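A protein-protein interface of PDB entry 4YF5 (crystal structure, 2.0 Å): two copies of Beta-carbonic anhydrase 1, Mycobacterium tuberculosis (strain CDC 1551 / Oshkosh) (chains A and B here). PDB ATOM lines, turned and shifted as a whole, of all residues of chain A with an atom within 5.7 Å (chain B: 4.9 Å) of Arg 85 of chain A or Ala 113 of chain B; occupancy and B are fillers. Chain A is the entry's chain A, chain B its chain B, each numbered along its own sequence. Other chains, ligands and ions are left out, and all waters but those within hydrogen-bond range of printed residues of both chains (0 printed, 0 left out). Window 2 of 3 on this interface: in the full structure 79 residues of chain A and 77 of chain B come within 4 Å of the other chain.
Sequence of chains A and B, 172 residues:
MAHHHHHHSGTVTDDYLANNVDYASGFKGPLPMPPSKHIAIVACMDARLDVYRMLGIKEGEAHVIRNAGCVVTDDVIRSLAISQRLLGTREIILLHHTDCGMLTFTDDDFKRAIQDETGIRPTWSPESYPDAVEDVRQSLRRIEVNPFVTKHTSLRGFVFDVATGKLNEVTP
OE1 of Glu 117 of chain B is in salt-bridge range of NH1 of Arg 85 of chain A, at 2.6 Å.
OE1 of Gln 84 of chain A lies within hydrogen-bond range of N of Lys 151 of chain A.
Phe 110 of chain B touches Ile 82 of chain A (CZ to CG1, 3.8 Å).
NH2 of Arg 85 of chain A touches CB of Ala 113 of chain B, at 3.9 Å.
Arg 85 of chain A touches Ile 114 of chain B.
Leu 86 of chain A touches Phe 110 of chain B (CG to CE1, 3.6 Å).
Phe 148 of chain A touches Ile 114 of chain B.
Glu 117 of chain B touches Lys 151 of chain A (OE1 to CE, 3.8 Å).
Leu 80 of chain A touches none of the printed residues of chain B.
Printed residues of chain B within 4 Å of Arg 85 of chain A: Ala 113 (3.9 Å), Ile 114 (3.6 Å) and Glu 117 (2.6 Å).
Printed residues of chain B within 4 Å of Phe 148 of chain A: Ile 114.
Printed residues of chain B within 4 Å of Lys 151 of chain A: Glu 117 (3.8 Å).
Lys 111 of chain B touches none of the printed residues of chain A.
Ala 113 of chain B touches just one residue of chain A: Arg 85 (3.9 Å).
The nearest residue of chain B that does not touch Arg 85 of chain A is Phe 110 of chain B (4.1 Å).
The nearest printed residue of chain A that does not touch Ala 113 of chain B is Leu 86 of chain A (7.0 Å).
The nearest printed residue of chain A that does not touch Ile 114 of chain B is Ala 81 of chain A (4.8 Å).
Hydrophobic or aromatic side chains of chain A that line the printed part of chain B: Ile 82, Leu 86 and Phe 148.
Hydrophobic or aromatic side chains of chain B within 4 Å of the printed part of chain A: Phe 110, Ala 113 and Ile 114.
Among the printed residues, 7 pairs touch across the chains.
Among the printed residues, Asp or Glu carboxylates within 4 Å of a Lys or Arg side-chain nitrogen of the other chain: Arg 85 of chain A with Glu 117 of chain B (2.6 Å).
No position is printed for both chains.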
ATOM      1  N   LEU A  80      16.695   6.445   9.327  1.00  0.00           N
ATOM      2  CA  LEU A  80      16.588   5.155   8.672  1.00  0.00           C
ATOM      3  C   LEU A  80      17.471   4.115   9.353  1.00  0.00           C
ATOM      4  O   LEU A  80      17.081   2.958   9.514  1.00  0.00           O
ATOM      5  CB  LEU A  80      16.961   5.292   7.202  1.00  0.00           C
ATOM      6  CG  LEU A  80      15.961   5.955   6.265  1.00  0.00           C
ATOM      7  CD1 LEU A  80      16.664   6.201   4.954  1.00  0.00           C
ATOM      8  CD2 LEU A  80      14.740   5.064   6.050  1.00  0.00           C
ATOM      9  N   ALA A  81      18.670   4.531   9.738  1.00  0.00           N
ATOM     10  CA  ALA A  81      19.572   3.668  10.473  1.00  0.00           C
ATOM     11  C   ALA A  81      18.901   3.188  11.752  1.00  0.00           C
ATOM     12  O   ALA A  81      18.894   1.982  12.054  1.00  0.00           O
ATOM     13  CB  ALA A  81      20.891   4.403  10.783  1.00  0.00           C
ATOM     14  N   ILE A  82      18.313   4.128  12.492  1.00  0.00           N
ATOM     15  CA  ILE A  82      17.646   3.785  13.736  1.00  0.00           C
ATOM     16  C   ILE A  82      16.484   2.843  13.417  1.00  0.00           C
ATOM     17  O   ILE A  82      16.330   1.810  14.064  1.00  0.00           O
ATOM     18  CB  ILE A  82      17.155   5.026  14.489  1.00  0.00           C
ATOM     19  CG1 ILE A  82      18.359   5.795  15.043  1.00  0.00           C
ATOM     20  CG2 ILE A  82      16.214   4.628  15.628  1.00  0.00           C
ATOM     21  CD1 ILE A  82      18.011   7.181  15.613  1.00  0.00           C
ATOM     22  N   SER A  83      15.725   3.181  12.375  1.00  0.00           N
ATOM     23  CA  SER A  83      14.588   2.381  11.945  1.00  0.00           C
ATOM     24  C   SER A  83      14.967   0.934  11.668  1.00  0.00           C
ATOM     25  O   SER A  83      14.352   0.021  12.220  1.00  0.00           O
ATOM     26  CB  SER A  83      13.957   2.976  10.690  1.00  0.00           C
ATOM     27  OG  SER A  83      12.771   2.264  10.363  1.00  0.00           O
ATOM     28  N   GLN A  84      15.964   0.732  10.806  1.00  0.00           N
ATOM     29  CA  GLN A  84      16.407  -0.619  10.458  1.00  0.00           C
ATOM     30  C   GLN A  84      17.144  -1.345  11.587  1.00  0.00           C
ATOM     31  O   GLN A  84      16.787  -2.467  11.943  1.00  0.00           O
ATOM     32  CB  GLN A  84      17.314  -0.590   9.223  1.00  0.00           C
ATOM     33  CG  GLN A  84      16.654  -0.026   7.990  1.00  0.00           C
ATOM     34  CD  GLN A  84      17.540  -0.128   6.774  1.00  0.00           C
ATOM     35  OE1 GLN A  84      18.733  -0.434   6.881  1.00  0.00           O
ATOM     36  NE2 GLN A  84      16.968   0.127   5.608  1.00  0.00           N
ATOM     37  N   ARG A  85      18.191  -0.727  12.127  1.00  0.00           N
ATOM     38  CA  ARG A  85      19.027  -1.406  13.113  1.00  0.00           C
ATOM     39  C   ARG A  85      18.316  -1.691  14.441  1.00  0.00           C
ATOM     40  O   ARG A  85      18.503  -2.756  15.028  1.00  0.00           O
ATOM     41  CB  ARG A  85      20.297  -0.603  13.392  1.00  0.00           C
ATOM     42  CG  ARG A  85      21.150  -0.313  12.175  1.00  0.00           C
ATOM     43  CD  ARG A  85      22.432   0.366  12.600  1.00  0.00           C
ATOM     44  NE  ARG A  85      23.070  -0.394  13.670  1.00  0.00           N
ATOM     45  CZ  ARG A  85      23.889  -1.423  13.468  1.00  0.00           C
ATOM     46  NH1 ARG A  85      24.174  -1.810  12.230  1.00  0.00           N
ATOM     47  NH2 ARG A  85      24.425  -2.056  14.500  1.00  0.00           N
ATOM     48  N   LEU A  86      17.504  -0.752  14.916  1.00  0.00           N
ATOM     49  CA  LEU A  86      16.879  -0.912  16.226  1.00  0.00           C
ATOM     50  C   LEU A  86      15.418  -1.356  16.204  1.00  0.00           C
ATOM     51  O   LEU A  86      14.908  -1.820  17.221  1.00  0.00           O
ATOM     52  CB  LEU A  86      16.965   0.395  17.017  1.00  0.00           C
ATOM     53  CG  LEU A  86      18.322   0.987  17.421  1.00  0.00           C
ATOM     54  CD1 LEU A  86      18.075   2.127  18.402  1.00  0.00           C
ATOM     55  CD2 LEU A  86      19.274  -0.061  18.020  1.00  0.00           C
ATOM     56  N   LEU A  87      14.732  -1.189  15.074  1.00  0.00           N
ATOM     57  CA  LEU A  87      13.289  -1.446  15.031  1.00  0.00           C
ATOM     58  C   LEU A  87      12.884  -2.308  13.844  1.00  0.00           C
ATOM     59  O   LEU A  87      11.710  -2.354  13.467  1.00  0.00           O
ATOM     60  CB  LEU A  87      12.504  -0.120  15.018  1.00  0.00           C
ATOM     61  CG  LEU A  87      12.546   0.663  16.335  1.00  0.00           C
ATOM     62  CD1 LEU A  87      12.045   2.103  16.190  1.00  0.00           C
ATOM     63  CD2 LEU A  87      11.746  -0.060  17.405  1.00  0.00           C
ATOM     64  N   GLY A  88      13.868  -2.961  13.240  1.00  0.00           N
ATOM     65  CA  GLY A  88      13.630  -4.037  12.292  1.00  0.00           C
ATOM     66  C   GLY A  88      12.919  -3.728  10.986  1.00  0.00           C
ATOM     67  O   GLY A  88      12.287  -4.618  10.429  1.00  0.00           O
ATOM     68  N   PHE A 148      25.496   2.946   6.360  1.00  0.00           N
ATOM     69  CA  PHE A 148      24.744   2.672   7.581  1.00  0.00           C
ATOM     70  C   PHE A 148      23.307   2.226   7.314  1.00  0.00           C
ATOM     71  O   PHE A 148      22.619   1.762   8.221  1.00  0.00           O
ATOM     72  CB  PHE A 148      24.759   3.911   8.487  1.00  0.00           C
ATOM     73  CG  PHE A 148      26.140   4.490   8.680  1.00  0.00           C
ATOM     74  CD1 PHE A 148      26.418   5.804   8.348  1.00  0.00           C
ATOM     75  CD2 PHE A 148      27.167   3.701   9.168  1.00  0.00           C
ATOM     76  CE1 PHE A 148      27.703   6.323   8.511  1.00  0.00           C
ATOM     77  CE2 PHE A 148      28.441   4.214   9.352  1.00  0.00           C
ATOM     78  CZ  PHE A 148      28.707   5.531   9.022  1.00  0.00           C
ATOM     79  N   LYS A 151      20.307  -2.629   5.599  1.00  0.00           N
ATOM     80  CA  LYS A 151      19.450  -3.738   6.025  1.00  0.00           C
ATOM     81  C   LYS A 151      18.115  -3.808   5.280  1.00  0.00           C
ATOM     82  O   LYS A 151      17.169  -4.426   5.770  1.00  0.00           O
ATOM     83  CB  LYS A 151      19.167  -3.648   7.539  1.00  0.00           C
ATOM     84  CG  LYS A 151      20.407  -3.709   8.444  1.00  0.00           C
ATOM     85  CD  LYS A 151      21.050  -5.099   8.432  1.00  0.00           C
ATOM     86  CE  LYS A 151      22.574  -5.043   8.483  1.00  0.00           C
ATOM     87  NZ  LYS A 151      23.183  -5.070   7.120  1.00  0.00           N
ATOM     88  N   ASP B 109      26.751   4.376  22.440  1.00  0.00           N
ATOM     89  CA  ASP B 109      26.533   2.936  22.306  1.00  0.00           C
ATOM     90  C   ASP B 109      26.099   2.578  20.896  1.00  0.00           C
ATOM     91  O   ASP B 109      26.594   1.616  20.304  1.00  0.00           O
ATOM     92  CB  ASP B 109      25.479   2.445  23.302  1.00  0.00           C
ATOM     93  CG  ASP B 109      26.036   2.269  24.694  1.00  0.00           C
ATOM     94  OD1 ASP B 109      27.254   2.017  24.813  1.00  0.00           O
ATOM     95  OD2 ASP B 109      25.258   2.376  25.666  1.00  0.00           O
ATOM     96  N   PHE B 110      25.177   3.373  20.368  1.00  0.00           N
ATOM     97  CA  PHE B 110      24.607   3.135  19.049  1.00  0.00           C
ATOM     98  C   PHE B 110      25.701   3.234  18.002  1.00  0.00           C
ATOM     99  O   PHE B 110      25.859   2.341  17.170  1.00  0.00           O
ATOM    100  CB  PHE B 110      23.480   4.133  18.774  1.00  0.00           C
ATOM    101  CG  PHE B 110      22.758   3.908  17.473  1.00  0.00           C
ATOM    102  CD1 PHE B 110      21.956   2.785  17.289  1.00  0.00           C
ATOM    103  CD2 PHE B 110      22.868   4.829  16.438  1.00  0.00           C
ATOM    104  CE1 PHE B 110      21.284   2.577  16.085  1.00  0.00           C
ATOM    105  CE2 PHE B 110      22.203   4.635  15.230  1.00  0.00           C
ATOM    106  CZ  PHE B 110      21.404   3.508  15.052  1.00  0.00           C
ATOM    107  N   LYS B 111      26.466   4.317  18.080  1.00  0.00           N
ATOM    108  CA  LYS B 111      27.574   4.574  17.172  1.00  0.00           C
ATOM    109  C   LYS B 111      28.661   3.512  17.259  1.00  0.00           C
ATOM    110  O   LYS B 111      29.249   3.148  16.246  1.00  0.00           O
ATOM    111  CB  LYS B 111      28.182   5.953  17.455  1.00  0.00           C
ATOM    112  CG  LYS B 111      27.305   7.096  16.984  1.00  0.00           C
ATOM    113  CD  LYS B 111      27.981   8.435  17.189  1.00  0.00           C
ATOM    114  CE  LYS B 111      28.287   9.103  15.866  1.00  0.00           C
ATOM    115  NZ  LYS B 111      28.734  10.513  16.056  1.00  0.00           N
ATOM    116  N   ARG B 112      28.931   3.021  18.466  1.00  0.00           N
ATOM    117  CA  ARG B 112      29.919   1.954  18.624  1.00  0.00           C
ATOM    118  C   ARG B 112      29.456   0.696  17.908  1.00  0.00           C
ATOM    119  O   ARG B 112      30.221   0.104  17.149  1.00  0.00           O
ATOM    120  CB  ARG B 112      30.195   1.661  20.098  1.00  0.00           C
ATOM    121  CG  ARG B 112      31.470   0.842  20.333  1.00  0.00           C
ATOM    122  CD  ARG B 112      31.961   0.942  21.780  1.00  0.00           C
ATOM    123  NE  ARG B 112      30.963   0.499  22.754  1.00  0.00           N
ATOM    124  CZ  ARG B 112      30.307   1.307  23.586  1.00  0.00           C
ATOM    125  NH1 ARG B 112      30.539   2.617  23.577  1.00  0.00           N
ATOM    126  NH2 ARG B 112      29.418   0.802  24.432  1.00  0.00           N
ATOM    127  N   ALA B 113      28.204   0.299  18.135  1.00  0.00           N
ATOM    128  CA  ALA B 113      27.638  -0.860  17.442  1.00  0.00           C
ATOM    129  C   ALA B 113      27.829  -0.736  15.931  1.00  0.00           C
ATOM    130  O   ALA B 113      28.256  -1.673  15.257  1.00  0.00           O
ATOM    131  CB  ALA B 113      26.167  -1.011  17.777  1.00  0.00           C
ATOM    132  N   ILE B 114      27.524   0.447  15.413  1.00  0.00           N
ATOM    133  CA  ILE B 114      27.616   0.728  13.985  1.00  0.00           C
ATOM    134  C   ILE B 114      29.056   0.585  13.511  1.00  0.00           C
ATOM    135  O   ILE B 114      29.332  -0.085  12.511  1.00  0.00           O
ATOM    136  CB  ILE B 114      27.081   2.155  13.664  1.00  0.00           C
ATOM    137  CG1 ILE B 114      25.561   2.200  13.829  1.00  0.00           C
ATOM    138  CG2 ILE B 114      27.408   2.547  12.252  1.00  0.00           C
ATOM    139  CD1 ILE B 114      24.907   3.501  13.287  1.00  0.00           C
ATOM    140  N   GLN B 115      29.977   1.205  14.244  1.00  0.00           N
ATOM    141  CA  GLN B 115      31.393   1.139  13.898  1.00  0.00           C
ATOM    142  C   GLN B 115      31.929  -0.293  13.988  1.00  0.00           C
ATOM    143  O   GLN B 115      32.707  -0.721  13.131  1.00  0.00           O
ATOM    144  CB  GLN B 115      32.228   2.062  14.800  1.00  0.00           C
ATOM    145  CG  GLN B 115      33.702   2.021  14.454  1.00  0.00           C
ATOM    146  CD  GLN B 115      34.528   3.081  15.143  1.00  0.00           C
ATOM    147  OE1 GLN B 115      33.996   3.967  15.804  1.00  0.00           O
ATOM    148  NE2 GLN B 115      35.847   2.997  14.983  1.00  0.00           N
ATOM    149  N   ASP B 116      31.518  -1.032  15.015  1.00  0.00           N
ATOM    150  CA  ASP B 116      31.911  -2.446  15.106  1.00  0.00           C
ATOM    151  C   ASP B 116      31.477  -3.208  13.855  1.00  0.00           C
ATOM    152  O   ASP B 116      32.240  -3.973  13.276  1.00  0.00           O
ATOM    153  CB  ASP B 116      31.312  -3.112  16.345  1.00  0.00           C
ATOM    154  CG  ASP B 116      32.115  -2.841  17.596  1.00  0.00           C
ATOM    155  OD1 ASP B 116      33.271  -2.383  17.469  1.00  0.00           O
ATOM    156  OD2 ASP B 116      31.590  -3.091  18.704  1.00  0.00           O
ATOM    157  N   GLU B 117      30.246  -2.961  13.429  1.00  0.00           N
ATOM    158  CA  GLU B 117      29.659  -3.655  12.293  1.00  0.00           C
ATOM    159  C   GLU B 117      30.256  -3.231  10.957  1.00  0.00           C
ATOM    160  O   GLU B 117      30.568  -4.078  10.123  1.00  0.00           O
ATOM    161  CB  GLU B 117      28.161  -3.408  12.292  1.00  0.00           C
ATOM    162  CG  GLU B 117      27.332  -4.394  11.531  1.00  0.00           C
ATOM    163  CD  GLU B 117      25.898  -4.351  11.999  1.00  0.00           C
ATOM    164  OE1 GLU B 117      25.007  -4.067  11.170  1.00  0.00           O
ATOM    165  OE2 GLU B 117      25.673  -4.577  13.209  1.00  0.00           O
